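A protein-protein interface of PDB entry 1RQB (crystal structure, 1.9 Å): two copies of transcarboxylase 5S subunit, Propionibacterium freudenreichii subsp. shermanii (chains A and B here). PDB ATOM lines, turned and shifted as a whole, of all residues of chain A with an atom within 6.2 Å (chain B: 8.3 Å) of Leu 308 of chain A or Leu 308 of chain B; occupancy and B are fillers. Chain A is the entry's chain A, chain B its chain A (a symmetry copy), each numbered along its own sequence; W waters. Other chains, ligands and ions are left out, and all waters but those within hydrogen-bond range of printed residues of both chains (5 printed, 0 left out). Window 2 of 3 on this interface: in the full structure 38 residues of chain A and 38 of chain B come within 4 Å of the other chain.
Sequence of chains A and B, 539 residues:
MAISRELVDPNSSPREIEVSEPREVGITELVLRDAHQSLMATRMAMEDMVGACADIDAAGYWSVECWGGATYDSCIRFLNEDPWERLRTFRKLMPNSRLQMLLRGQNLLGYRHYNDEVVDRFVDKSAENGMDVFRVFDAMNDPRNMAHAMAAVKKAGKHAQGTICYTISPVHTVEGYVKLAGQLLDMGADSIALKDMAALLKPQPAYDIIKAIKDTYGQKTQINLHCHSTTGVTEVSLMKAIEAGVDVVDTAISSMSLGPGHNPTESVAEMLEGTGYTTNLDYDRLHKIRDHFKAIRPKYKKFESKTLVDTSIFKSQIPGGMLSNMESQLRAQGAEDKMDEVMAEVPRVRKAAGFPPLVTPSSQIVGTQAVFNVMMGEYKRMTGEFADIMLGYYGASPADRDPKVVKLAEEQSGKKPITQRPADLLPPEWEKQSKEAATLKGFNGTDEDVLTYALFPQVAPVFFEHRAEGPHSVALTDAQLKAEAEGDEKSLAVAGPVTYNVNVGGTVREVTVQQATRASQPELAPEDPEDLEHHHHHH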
ATOM      1  N   SER A 229     -12.476 -24.630  -0.904  1.00  0.00           N
ATOM      2  CA  SER A 229     -12.636 -26.002  -0.399  1.00  0.00           C
ATOM      3  C   SER A 229     -13.875 -26.138   0.487  1.00  0.00           C
ATOM      4  O   SER A 229     -14.020 -27.122   1.212  1.00  0.00           O
ATOM      5  CB  SER A 229     -11.400 -26.376   0.420  1.00  0.00           C
ATOM      6  OG  SER A 229     -11.132 -25.351   1.384  1.00  0.00           O
ATOM      7  N   THR A 230     -14.773 -25.169   0.397  1.00  0.00           N
ATOM      8  CA  THR A 230     -15.984 -25.078   1.226  1.00  0.00           C
ATOM      9  C   THR A 230     -16.828 -26.356   1.274  1.00  0.00           C
ATOM     10  O   THR A 230     -17.359 -26.701   2.330  1.00  0.00           O
ATOM     11  CB  THR A 230     -16.849 -23.913   0.739  1.00  0.00           C
ATOM     12  OG1 THR A 230     -15.988 -22.805   0.433  1.00  0.00           O
ATOM     13  CG2 THR A 230     -17.849 -23.494   1.829  1.00  0.00           C
ATOM     14  N   THR A 231     -16.984 -27.050   0.154  1.00  0.00           N
ATOM     15  CA  THR A 231     -17.814 -28.263   0.094  1.00  0.00           C
ATOM     16  C   THR A 231     -16.980 -29.530   0.298  1.00  0.00           C
ATOM     17  O   THR A 231     -17.529 -30.629   0.353  1.00  0.00           O
ATOM     18  CB  THR A 231     -18.462 -28.407  -1.269  1.00  0.00           C
ATOM     19  OG1 THR A 231     -17.425 -28.402  -2.263  1.00  0.00           O
ATOM     20  CG2 THR A 231     -19.439 -27.272  -1.510  1.00  0.00           C
ATOM     21  N   GLY A 232     -15.663 -29.387   0.344  1.00  0.00           N
ATOM     22  CA  GLY A 232     -14.801 -30.543   0.538  1.00  0.00           C
ATOM     23  C   GLY A 232     -14.574 -31.468  -0.650  1.00  0.00           C
ATOM     24  O   GLY A 232     -13.957 -32.517  -0.471  1.00  0.00           O
ATOM     25  N   SER A 254      -0.726 -24.670   3.905  1.00  0.00           N
ATOM     26  CA  SER A 254      -1.531 -25.553   4.763  1.00  0.00           C
ATOM     27  C   SER A 254      -1.991 -24.948   6.094  1.00  0.00           C
ATOM     28  O   SER A 254      -3.075 -25.295   6.560  1.00  0.00           O
ATOM     29  CB  SER A 254      -0.809 -26.895   4.990  1.00  0.00           C
ATOM     30  OG  SER A 254       0.378 -26.739   5.737  1.00  0.00           O
ATOM     31  N   SER A 257      -5.466 -22.916   5.320  1.00  0.00           N
ATOM     32  CA  SER A 257      -6.253 -23.580   4.271  1.00  0.00           C
ATOM     33  C   SER A 257      -7.490 -24.282   4.838  1.00  0.00           C
ATOM     34  O   SER A 257      -7.699 -24.334   6.050  1.00  0.00           O
ATOM     35  CB  SER A 257      -5.382 -24.637   3.579  1.00  0.00           C
ATOM     36  OG  SER A 257      -5.111 -25.708   4.472  1.00  0.00           O
ATOM     37  N   LEU A 258      -8.292 -24.816   3.908  1.00  0.00           N
ATOM     38  CA  LEU A 258      -9.522 -25.587   4.147  1.00  0.00           C
ATOM     39  C   LEU A 258     -10.693 -24.707   4.590  1.00  0.00           C
ATOM     40  O   LEU A 258     -10.564 -23.494   4.746  1.00  0.00           O
ATOM     41  CB  LEU A 258      -9.275 -26.723   5.148  1.00  0.00           C
ATOM     42  CG  LEU A 258      -8.210 -27.715   4.652  1.00  0.00           C
ATOM     43  CD1 LEU A 258      -8.120 -28.895   5.608  1.00  0.00           C
ATOM     44  CD2 LEU A 258      -8.551 -28.195   3.255  1.00  0.00           C
ATOM     45  N   GLY A 259     -11.850 -25.335   4.773  1.00  0.00           N
ATOM     46  CA  GLY A 259     -13.033 -24.575   5.138  1.00  0.00           C
ATOM     47  C   GLY A 259     -13.425 -23.688   3.964  1.00  0.00           C
ATOM     48  O   GLY A 259     -13.321 -24.112   2.814  1.00  0.00           O
ATOM     49  N   PRO A 260     -13.862 -22.442   4.216  1.00  0.00           N
ATOM     50  CA  PRO A 260     -14.272 -21.484   3.175  1.00  0.00           C
ATOM     51  C   PRO A 260     -13.053 -20.989   2.394  1.00  0.00           C
ATOM     52  O   PRO A 260     -13.174 -20.180   1.474  1.00  0.00           O
ATOM     53  CB  PRO A 260     -14.911 -20.341   3.959  1.00  0.00           C
ATOM     54  CG  PRO A 260     -15.130 -20.880   5.330  1.00  0.00           C
ATOM     55  CD  PRO A 260     -14.035 -21.865   5.558  1.00  0.00           C
ATOM     56  N   ARG A 297      -1.693 -17.176  12.890  1.00  0.00           N
ATOM     57  CA  ARG A 297      -3.147 -17.348  12.752  1.00  0.00           C
ATOM     58  C   ARG A 297      -3.936 -17.284  14.063  1.00  0.00           C
ATOM     59  O   ARG A 297      -5.031 -16.723  14.086  1.00  0.00           O
ATOM     60  CB  ARG A 297      -3.463 -18.634  12.000  1.00  0.00           C
ATOM     61  CG  ARG A 297      -4.946 -18.784  11.699  1.00  0.00           C
ATOM     62  CD  ARG A 297      -5.196 -19.983  10.823  1.00  0.00           C
ATOM     63  NE  ARG A 297      -6.614 -20.126  10.539  1.00  0.00           N
ATOM     64  CZ  ARG A 297      -7.115 -21.053   9.731  1.00  0.00           C
ATOM     65  NH1 ARG A 297      -6.299 -21.912   9.118  1.00  0.00           N
ATOM     66  NH2 ARG A 297      -8.425 -21.135   9.552  1.00  0.00           N
ATOM     67  N   LYS A 306     -16.867 -20.949  11.672  1.00  0.00           N
ATOM     68  CA  LYS A 306     -17.039 -22.171  12.471  1.00  0.00           C
ATOM     69  C   LYS A 306     -17.424 -23.406  11.651  1.00  0.00           C
ATOM     70  O   LYS A 306     -17.739 -24.441  12.235  1.00  0.00           O
ATOM     71  CB  LYS A 306     -18.093 -21.913  13.549  1.00  0.00           C
ATOM     72  CG  LYS A 306     -17.683 -20.820  14.534  1.00  0.00           C
ATOM     73  CD  LYS A 306     -18.784 -20.487  15.531  1.00  0.00           C
ATOM     74  CE  LYS A 306     -19.986 -19.864  14.843  1.00  0.00           C
ATOM     75  NZ  LYS A 306     -19.644 -18.539  14.241  1.00  0.00           N
ATOM     76  N   THR A 307     -17.401 -23.354  10.322  1.00  0.00           N
ATOM     77  CA  THR A 307     -17.775 -24.556   9.560  1.00  0.00           C
ATOM     78  C   THR A 307     -16.656 -24.934   8.587  1.00  0.00           C
ATOM     79  O   THR A 307     -16.253 -24.127   7.752  1.00  0.00           O
ATOM     80  CB  THR A 307     -19.091 -24.347   8.756  1.00  0.00           C
ATOM     81  OG1 THR A 307     -20.118 -23.842   9.625  1.00  0.00           O
ATOM     82  CG2 THR A 307     -19.563 -25.679   8.156  1.00  0.00           C
ATOM     83  N   LEU A 308     -16.166 -26.169   8.682  1.00  0.00           N
ATOM     84  CA  LEU A 308     -15.076 -26.624   7.806  1.00  0.00           C
ATOM     85  C   LEU A 308     -15.617 -27.178   6.487  1.00  0.00           C
ATOM     86  O   LEU A 308     -15.019 -26.984   5.430  1.00  0.00           O
ATOM     87  CB  LEU A 308     -14.240 -27.711   8.483  1.00  0.00           C
ATOM     88  CG  LEU A 308     -13.099 -27.257   9.392  1.00  0.00           C
ATOM     89  CD1 LEU A 308     -12.284 -28.473   9.812  1.00  0.00           C
ATOM     90  CD2 LEU A 308     -12.210 -26.253   8.644  1.00  0.00           C
ATOM     91  N   VAL A 309     -16.739 -27.880   6.544  1.00  0.00           N
ATOM     92  CA  VAL A 309     -17.295 -28.485   5.325  1.00  0.00           C
ATOM     93  C   VAL A 309     -18.812 -28.298   5.297  1.00  0.00           C
ATOM     94  O   VAL A 309     -19.500 -28.596   6.272  1.00  0.00           O
ATOM     95  CB  VAL A 309     -17.020 -30.009   5.279  1.00  0.00           C
ATOM     96  CG1 VAL A 309     -17.603 -30.621   3.983  1.00  0.00           C
ATOM     97  CG2 VAL A 309     -15.545 -30.272   5.378  1.00  0.00           C
ATOM     98  N   ASP A 310     -19.318 -27.824   4.164  1.00  0.00           N
ATOM     99  CA  ASP A 310     -20.762 -27.619   3.981  1.00  0.00           C
ATOM    100  C   ASP A 310     -21.115 -27.998   2.541  1.00  0.00           C
ATOM    101  O   ASP A 310     -20.693 -27.319   1.606  1.00  0.00           O
ATOM    102  CB  ASP A 310     -21.117 -26.151   4.244  1.00  0.00           C
ATOM    103  CG  ASP A 310     -22.618 -25.901   4.240  1.00  0.00           C
ATOM    104  OD1 ASP A 310     -23.391 -26.874   4.052  1.00  0.00           O
ATOM    105  OD2 ASP A 310     -23.022 -24.728   4.427  1.00  0.00           O
ATOM    106  N   LEU B  39     -10.587 -37.016  16.897  1.00  0.00           N
ATOM    107  CA  LEU B  39     -10.739 -35.557  16.994  1.00  0.00           C
ATOM    108  C   LEU B  39     -10.938 -35.047  18.424  1.00  0.00           C
ATOM    109  O   LEU B  39     -10.623 -33.890  18.701  1.00  0.00           O
ATOM    110  CB  LEU B  39     -11.918 -35.105  16.131  1.00  0.00           C
ATOM    111  CG  LEU B  39     -11.688 -35.254  14.623  1.00  0.00           C
ATOM    112  CD1 LEU B  39     -12.978 -35.039  13.873  1.00  0.00           C
ATOM    113  CD2 LEU B  39     -10.615 -34.258  14.181  1.00  0.00           C
ATOM    114  N   SER B 229      -7.342 -38.043   7.303  1.00  0.00           N
ATOM    115  CA  SER B 229      -7.143 -36.899   6.399  1.00  0.00           C
ATOM    116  C   SER B 229      -6.041 -35.966   6.901  1.00  0.00           C
ATOM    117  O   SER B 229      -5.922 -34.833   6.436  1.00  0.00           O
ATOM    118  CB  SER B 229      -8.451 -36.112   6.300  1.00  0.00           C
ATOM    119  OG  SER B 229      -8.943 -35.828   7.615  1.00  0.00           O
ATOM    120  N   THR B 230      -5.225 -36.459   7.819  1.00  0.00           N
ATOM    121  CA  THR B 230      -4.160 -35.692   8.485  1.00  0.00           C
ATOM    122  C   THR B 230      -3.228 -34.931   7.537  1.00  0.00           C
ATOM    123  O   THR B 230      -2.831 -33.806   7.840  1.00  0.00           O
ATOM    124  CB  THR B 230      -3.335 -36.629   9.370  1.00  0.00           C
ATOM    125  OG1 THR B 230      -4.232 -37.526  10.043  1.00  0.00           O
ATOM    126  CG2 THR B 230      -2.545 -35.822  10.414  1.00  0.00           C
ATOM    127  N   THR B 231      -2.851 -35.526   6.412  1.00  0.00           N
ATOM    128  CA  THR B 231      -1.922 -34.891   5.464  1.00  0.00           C
ATOM    129  C   THR B 231      -2.666 -34.144   4.356  1.00  0.00           C
ATOM    130  O   THR B 231      -2.041 -33.493   3.521  1.00  0.00           O
ATOM    131  CB  THR B 231      -1.071 -35.932   4.764  1.00  0.00           C
ATOM    132  OG1 THR B 231      -1.947 -36.875   4.126  1.00  0.00           O
ATOM    133  CG2 THR B 231      -0.168 -36.633   5.762  1.00  0.00           C
ATOM    134  N   GLY B 232      -3.984 -34.288   4.307  1.00  0.00           N
ATOM    135  CA  GLY B 232      -4.765 -33.607   3.285  1.00  0.00           C
ATOM    136  C   GLY B 232      -4.735 -34.176   1.873  1.00  0.00           C
ATOM    137  O   GLY B 232      -5.281 -33.542   0.972  1.00  0.00           O
ATOM    138  N   SER B 254     -19.626 -34.891   7.913  1.00  0.00           N
ATOM    139  CA  SER B 254     -18.884 -33.638   7.698  1.00  0.00           C
ATOM    140  C   SER B 254     -18.678 -32.766   8.940  1.00  0.00           C
ATOM    141  O   SER B 254     -17.649 -32.098   9.032  1.00  0.00           O
ATOM    142  CB  SER B 254     -19.516 -32.824   6.553  1.00  0.00           C
ATOM    143  OG  SER B 254     -20.808 -32.362   6.881  1.00  0.00           O
ATOM    144  N   SER B 255     -19.598 -32.739   9.900  1.00  0.00           N
ATOM    145  CA  SER B 255     -19.400 -31.884  11.081  1.00  0.00           C
ATOM    146  C   SER B 255     -18.381 -32.486  12.054  1.00  0.00           C
ATOM    147  O   SER B 255     -18.002 -31.858  13.041  1.00  0.00           O
ATOM    148  CB  SER B 255     -20.735 -31.644  11.798  1.00  0.00           C
ATOM    149  OG  SER B 255     -21.463 -32.854  11.940  1.00  0.00           O
ATOM    150  N   MET B 256     -17.925 -33.700  11.779  1.00  0.00           N
ATOM    151  CA  MET B 256     -16.942 -34.395  12.627  1.00  0.00           C
ATOM    152  C   MET B 256     -15.853 -34.978  11.724  1.00  0.00           C
ATOM    153  O   MET B 256     -15.495 -36.145  11.880  1.00  0.00           O
ATOM    154  CB  MET B 256     -17.608 -35.575  13.323  1.00  0.00           C
ATOM    155  CG  MET B 256     -18.790 -35.224  14.170  1.00  0.00           C
ATOM    156  SD  MET B 256     -18.112 -34.644  15.861  1.00  0.00           S
ATOM    157  CE  MET B 256     -17.753 -36.396  16.644  1.00  0.00           C
ATOM    158  N   SER B 257     -15.311 -34.167  10.811  1.00  0.00           N
ATOM    159  CA  SER B 257     -14.325 -34.664   9.841  1.00  0.00           C
ATOM    160  C   SER B 257     -13.130 -33.716   9.700  1.00  0.00           C
ATOM    161  O   SER B 257     -13.097 -32.634  10.284  1.00  0.00           O
ATOM    162  CB  SER B 257     -14.992 -34.793   8.465  1.00  0.00           C
ATOM    163  OG  SER B 257     -15.300 -33.507   7.947  1.00  0.00           O
ATOM    164  N   LEU B 258     -12.158 -34.175   8.902  1.00  0.00           N
ATOM    165  CA  LEU B 258     -10.916 -33.475   8.539  1.00  0.00           C
ATOM    166  C   LEU B 258      -9.901 -33.443   9.684  1.00  0.00           C
ATOM    167  O   LEU B 258     -10.154 -33.936  10.782  1.00  0.00           O
ATOM    168  CB  LEU B 258     -11.210 -32.060   8.023  1.00  0.00           C
ATOM    169  CG  LEU B 258     -12.103 -32.073   6.771  1.00  0.00           C
ATOM    170  CD1 LEU B 258     -12.232 -30.661   6.217  1.00  0.00           C
ATOM    171  CD2 LEU B 258     -11.522 -32.997   5.720  1.00  0.00           C
ATOM    172  N   GLY B 259      -8.735 -32.870   9.406  1.00  0.00           N
ATOM    173  CA  GLY B 259      -7.687 -32.843  10.412  1.00  0.00           C
ATOM    174  C   GLY B 259      -7.202 -34.267  10.650  1.00  0.00           C
ATOM    175  O   GLY B 259      -7.100 -35.046   9.704  1.00  0.00           O
ATOM    176  N   PRO B 260      -6.914 -34.647  11.907  1.00  0.00           N
ATOM    177  CA  PRO B 260      -6.438 -35.990  12.275  1.00  0.00           C
ATOM    178  C   PRO B 260      -7.566 -37.015  12.136  1.00  0.00           C
ATOM    179  O   PRO B 260      -7.380 -38.204  12.393  1.00  0.00           O
ATOM    180  CB  PRO B 260      -6.020 -35.845  13.736  1.00  0.00           C
ATOM    181  CG  PRO B 260      -5.959 -34.377  13.983  1.00  0.00           C
ATOM    182  CD  PRO B 260      -6.989 -33.774  13.089  1.00  0.00           C
ATOM    183  N   GLY B 261      -8.736 -36.512  11.755  1.00  0.00           N
ATOM    184  CA  GLY B 261      -9.893 -37.349  11.543  1.00  0.00           C
ATOM    185  C   GLY B 261      -9.925 -37.932  10.139  1.00  0.00           C
ATOM    186  O   GLY B 261      -8.897 -38.375   9.631  1.00  0.00           O
ATOM    187  N   PRO B 264     -14.837 -36.273   4.733  1.00  0.00           N
ATOM    188  CA  PRO B 264     -16.284 -36.129   4.933  1.00  0.00           C
ATOM    189  C   PRO B 264     -17.183 -37.046   4.102  1.00  0.00           C
ATOM    190  O   PRO B 264     -17.055 -37.133   2.881  1.00  0.00           O
ATOM    191  CB  PRO B 264     -16.543 -34.638   4.638  1.00  0.00           C
ATOM    192  CG  PRO B 264     -15.159 -34.020   4.477  1.00  0.00           C
ATOM    193  CD  PRO B 264     -14.325 -35.135   3.950  1.00  0.00           C
ATOM    194  N   SER B 267     -19.073 -35.241   1.350  1.00  0.00           N
ATOM    195  CA  SER B 267     -18.174 -34.796   0.275  1.00  0.00           C
ATOM    196  C   SER B 267     -17.807 -35.982  -0.619  1.00  0.00           C
ATOM    197  O   SER B 267     -17.793 -35.868  -1.844  1.00  0.00           O
ATOM    198  CB  SER B 267     -16.909 -34.174   0.866  1.00  0.00           C
ATOM    199  OG  SER B 267     -17.230 -33.011   1.617  1.00  0.00           O
ATOM    200  N   ARG B 290     -25.495 -34.808  10.296  1.00  0.00           N
ATOM    201  CA  ARG B 290     -24.523 -33.706  10.305  1.00  0.00           C
ATOM    202  C   ARG B 290     -24.936 -32.635  11.318  1.00  0.00           C
ATOM    203  O   ARG B 290     -24.130 -32.202  12.139  1.00  0.00           O
ATOM    204  CB  ARG B 290     -24.440 -33.045   8.930  1.00  0.00           C
ATOM    205  CG  ARG B 290     -23.416 -31.934   8.907  1.00  0.00           C
ATOM    206  CD  ARG B 290     -23.396 -31.222   7.577  1.00  0.00           C
ATOM    207  NE  ARG B 290     -24.575 -30.394   7.379  1.00  0.00           N
ATOM    208  CZ  ARG B 290     -24.636 -29.111   7.723  1.00  0.00           C
ATOM    209  NH1 ARG B 290     -23.576 -28.527   8.281  1.00  0.00           N
ATOM    210  NH2 ARG B 290     -25.743 -28.408   7.498  1.00  0.00           N
ATOM    211  N   LYS B 294     -23.114 -31.304  14.697  1.00  0.00           N
ATOM    212  CA  LYS B 294     -22.632 -29.918  14.624  1.00  0.00           C
ATOM    213  C   LYS B 294     -23.011 -29.183  15.912  1.00  0.00           C
ATOM    214  O   LYS B 294     -22.259 -28.349  16.415  1.00  0.00           O
ATOM    215  CB  LYS B 294     -23.247 -29.193  13.423  1.00  0.00           C
ATOM    216  CG  LYS B 294     -22.765 -27.751  13.320  1.00  0.00           C
ATOM    217  CD  LYS B 294     -23.355 -27.010  12.131  1.00  0.00           C
ATOM    218  CE  LYS B 294     -22.829 -25.575  12.093  1.00  0.00           C
ATOM    219  NZ  LYS B 294     -21.330 -25.490  12.184  1.00  0.00           N
ATOM    220  N   ARG B 297     -20.626 -30.909  18.912  1.00  0.00           N
ATOM    221  CA  ARG B 297     -19.158 -30.818  18.910  1.00  0.00           C
ATOM    222  C   ARG B 297     -18.579 -29.659  19.728  1.00  0.00           C
ATOM    223  O   ARG B 297     -17.550 -29.832  20.381  1.00  0.00           O
ATOM    224  CB  ARG B 297     -18.628 -30.783  17.483  1.00  0.00           C
ATOM    225  CG  ARG B 297     -17.110 -30.840  17.424  1.00  0.00           C
ATOM    226  CD  ARG B 297     -16.633 -30.962  16.001  1.00  0.00           C
ATOM    227  NE  ARG B 297     -15.181 -31.012  15.946  1.00  0.00           N
ATOM    228  CZ  ARG B 297     -14.491 -31.192  14.827  1.00  0.00           C
ATOM    229  NH1 ARG B 297     -15.133 -31.351  13.668  1.00  0.00           N
ATOM    230  NH2 ARG B 297     -13.167 -31.194  14.861  1.00  0.00           N
ATOM    231  N   GLU B 304     -10.075 -30.791  21.668  1.00  0.00           N
ATOM    232  CA  GLU B 304      -9.763 -30.676  20.235  1.00  0.00           C
ATOM    233  C   GLU B 304      -8.270 -30.456  19.980  1.00  0.00           C
ATOM    234  O   GLU B 304      -7.533 -30.001  20.853  1.00  0.00           O
ATOM    235  CB  GLU B 304     -10.522 -29.498  19.618  1.00  0.00           C
ATOM    236  CG  GLU B 304     -12.030 -29.599  19.629  1.00  0.00           C
ATOM    237  CD  GLU B 304     -12.586 -30.280  18.383  1.00  0.00           C
ATOM    238  OE1 GLU B 304     -11.881 -30.323  17.351  1.00  0.00           O
ATOM    239  OE2 GLU B 304     -13.740 -30.756  18.431  1.00  0.00           O
ATOM    240  N   SER B 305      -7.850 -30.774  18.748  1.00  0.00           N
ATOM    241  CA  SER B 305      -6.468 -30.592  18.279  1.00  0.00           C
ATOM    242  C   SER B 305      -6.386 -29.257  17.536  1.00  0.00           C
ATOM    243  O   SER B 305      -7.409 -28.709  17.129  1.00  0.00           O
ATOM    244  CB  SER B 305      -6.060 -31.719  17.329  1.00  0.00           C
ATOM    245  OG  SER B 305      -5.840 -32.921  18.041  1.00  0.00           O
ATOM    246  N   LYS B 306      -5.174 -28.758  17.307  1.00  0.00           N
ATOM    247  CA  LYS B 306      -5.019 -27.438  16.678  1.00  0.00           C
ATOM    248  C   LYS B 306      -4.414 -27.482  15.271  1.00  0.00           C
ATOM    249  O   LYS B 306      -4.103 -26.429  14.718  1.00  0.00           O
ATOM    250  CB  LYS B 306      -4.160 -26.555  17.586  1.00  0.00           C
ATOM    251  CG  LYS B 306      -4.801 -26.301  18.949  1.00  0.00           C
ATOM    252  CD  LYS B 306      -3.891 -25.522  19.888  1.00  0.00           C
ATOM    253  CE  LYS B 306      -2.657 -26.327  20.259  1.00  0.00           C
ATOM    254  NZ  LYS B 306      -3.019 -27.545  21.049  1.00  0.00           N
ATOM    255  N   THR B 307      -4.246 -28.649  14.657  1.00  0.00           N
ATOM    256  CA  THR B 307      -3.664 -28.661  13.306  1.00  0.00           C
ATOM    257  C   THR B 307      -4.592 -29.398  12.337  1.00  0.00           C
ATOM    258  O   THR B 307      -4.935 -30.558  12.558  1.00  0.00           O
ATOM    259  CB  THR B 307      -2.267 -29.345  13.282  1.00  0.00           C
ATOM    260  OG1 THR B 307      -1.425 -28.770  14.295  1.00  0.00           O
ATOM    261  CG2 THR B 307      -1.601 -29.144  11.914  1.00  0.00           C
ATOM    262  N   LEU B 308      -4.985 -28.731  11.253  1.00  0.00           N
ATOM    263  CA  LEU B 308      -5.892 -29.343  10.271  1.00  0.00           C
ATOM    264  C   LEU B 308      -5.118 -30.147   9.225  1.00  0.00           C
ATOM    265  O   LEU B 308      -5.569 -31.202   8.782  1.00  0.00           O
ATOM    266  CB  LEU B 308      -6.724 -28.281   9.550  1.00  0.00           C
ATOM    267  CG  LEU B 308      -8.020 -27.828  10.220  1.00  0.00           C
ATOM    268  CD1 LEU B 308      -8.783 -26.919   9.264  1.00  0.00           C
ATOM    269  CD2 LEU B 308      -8.871 -29.054  10.581  1.00  0.00           C
ATOM    270  N   VAL B 309      -3.962 -29.647   8.816  1.00  0.00           N
ATOM    271  CA  VAL B 309      -3.183 -30.338   7.778  1.00  0.00           C
ATOM    272  C   VAL B 309      -1.700 -30.329   8.147  1.00  0.00           C
ATOM    273  O   VAL B 309      -1.140 -29.284   8.474  1.00  0.00           O
ATOM    274  CB  VAL B 309      -3.319 -29.626   6.408  1.00  0.00           C
ATOM    275  CG1 VAL B 309      -2.502 -30.378   5.329  1.00  0.00           C
ATOM    276  CG2 VAL B 309      -4.765 -29.533   6.015  1.00  0.00           C
ATOM    277  N   ASP B 310      -1.075 -31.498   8.069  1.00  0.00           N
ATOM    278  CA  ASP B 310       0.358 -31.637   8.366  1.00  0.00           C
ATOM    279  C   ASP B 310       0.950 -32.650   7.384  1.00  0.00           C
ATOM    280  O   ASP B 310       0.614 -33.832   7.442  1.00  0.00           O
ATOM    281  CB  ASP B 310       0.545 -32.127   9.807  1.00  0.00           C
ATOM    282  CG  ASP B 310       2.004 -32.131  10.240  1.00  0.00           C
ATOM    283  OD1 ASP B 310       2.876 -31.733   9.427  1.00  0.00           O
ATOM    284  OD2 ASP B 310       2.275 -32.532  11.397  1.00  0.00           O
ATOM    285  N   THR B 311       1.819 -32.190   6.480  1.00  0.00           N
ATOM    286  CA  THR B 311       2.429 -33.074   5.473  1.00  0.00           C
ATOM    287  C   THR B 311       3.892 -33.364   5.814  1.00  0.00           C
ATOM    288  O   THR B 311       4.594 -34.009   5.037  1.00  0.00           O
ATOM    289  CB  THR B 311       2.455 -32.423   4.068  1.00  0.00           C
ATOM    290  OG1 THR B 311       3.189 -31.200   4.148  1.00  0.00           O
ATOM    291  CG2 THR B 311       1.033 -32.138   3.532  1.00  0.00           C
HETATM  292  O   HOH W   1       1.743 -29.266   6.085  1.00  0.00           O
HETATM  293  O   HOH W   2     -20.339 -29.814   8.214  1.00  0.00           O
HETATM  294  O   HOH W   3      -0.496 -26.929   8.510  1.00  0.00           O
HETATM  295  O   HOH W   4      -3.732 -26.713   8.951  1.00  0.00           O
HETATM  296  O   HOH W   5     -17.233 -29.274   9.092  1.00  0.00           O
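Water W2 lies within hydrogen-bond range of the backbone carbonyl oxygen of Val 309 of chain A (2.4 Å), the side-chain hydroxyl of Ser 254 of chain B (2.9 Å), the backbone NH of Ser 255 of chain B (3.5 Å) and the guanidinium group of Arg 290 of chain B (3.5 Å).
Water W3 lies within hydrogen-bond range of the backbone carbonyl oxygen (O) of Val 309 of chain B (2.4 Å) and the side-chain hydroxyl (OG) of Ser 254 of chain A (2.9 Å).
The backbone carbonyl oxygen (O) of Thr 231 of chain A sits at hydrogen-bond distance from the side-chain hydroxyl (OG) of Ser 267 of chain B.
NZ of Lys 294 of chain B sits at hydrogen-bond distance from OG1 of Thr 307 of chain A.
The side-chain hydroxyl (OG) of Ser 257 of chain B is in hydrogen-bond range of the backbone carbonyl oxygen (O) of Ser 254 of chain B, 2.9 Å away.
The backbone carbonyl oxygen (O) of Ser 254 of chain A is in hydrogen-bond range of the side-chain hydroxyl (OG) of Ser 257 of chain A, 2.9 Å away.
Of the 26 printed residues of chain B, 7 touch a printed residue of chain A.
Hydrophobic or aromatic side chains of chain B that line the printed part of chain A: Leu 258, Pro 264, Leu 308 and Val 309.
Printed residues of chain A that touch a printed residue of chain B: Thr 231, Gly 232, Ser 254, Leu 258, Lys 306, Thr 307, Leu 308 and Val 309.
Among the printed residues, no Asp or Glu carboxylate lies within 4 Å of a Lys or Arg side-chain nitrogen of the other chain.
Among the printed residues, merely in contact across the chains: Gly 232 of chain A with Ser 267 of chain B (3.6 Å), Ser 254 of chain A with Val 309 of chain B (3.9 Å), Leu 258 of chain A with Val 309 of chain B (3.4 Å), Lys 306 of chain A with Lys 294 of chain B (3.7 Å), Leu 308 of chain A with Leu 308 of chain B (3.5 Å), Val 309 of chain A with Ser 254 of chain B (3.9 Å), Val 309 of chain A with Leu 258 of chain B (3.4 Å), Val 309 of chain A with Pro 264 of chain B (3.9 Å) and Val 309 of chain A with Ser 267 of chain B (3.4 Å).
Ser 254 of chain A touches Val 309 of chain B, and with the chains exchanged Val 309 of chain A touches Ser 254 of chain B.
Leu 258 of chain A touches Val 309 of chain B, and with the chains exchanged Val 309 of chain A touches Leu 258 of chain B.
Leu 308 of chain B touches its own counterpart, Leu 308 of chain A.
Positions printed for both chains: 229, 230, 231, 232, 254, 257, 258, 259, 260, 297, 306, 307, 308, 309 and 310.
Of the 11 pairs that touch across the chains among the printed residues, 5 have their exchanged pair printed and touching as well.
Of the printed residues of chain B, Gly 232 of chain A touches Ser 267 (3.6 Å).
No residue of chain B comes within 4 Å of Gly 259 of chain A.
Of chain B, only Leu 308 comes within 4 Å of Leu 308 of chain A.
Printed residues of chain A within 4 Å of Pro 264 of chain B: Val 309 (3.9 Å).
The nearest residue of chain A that does not touch Leu 308 of chain B is Leu 258 of chain A (4.1 Å).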
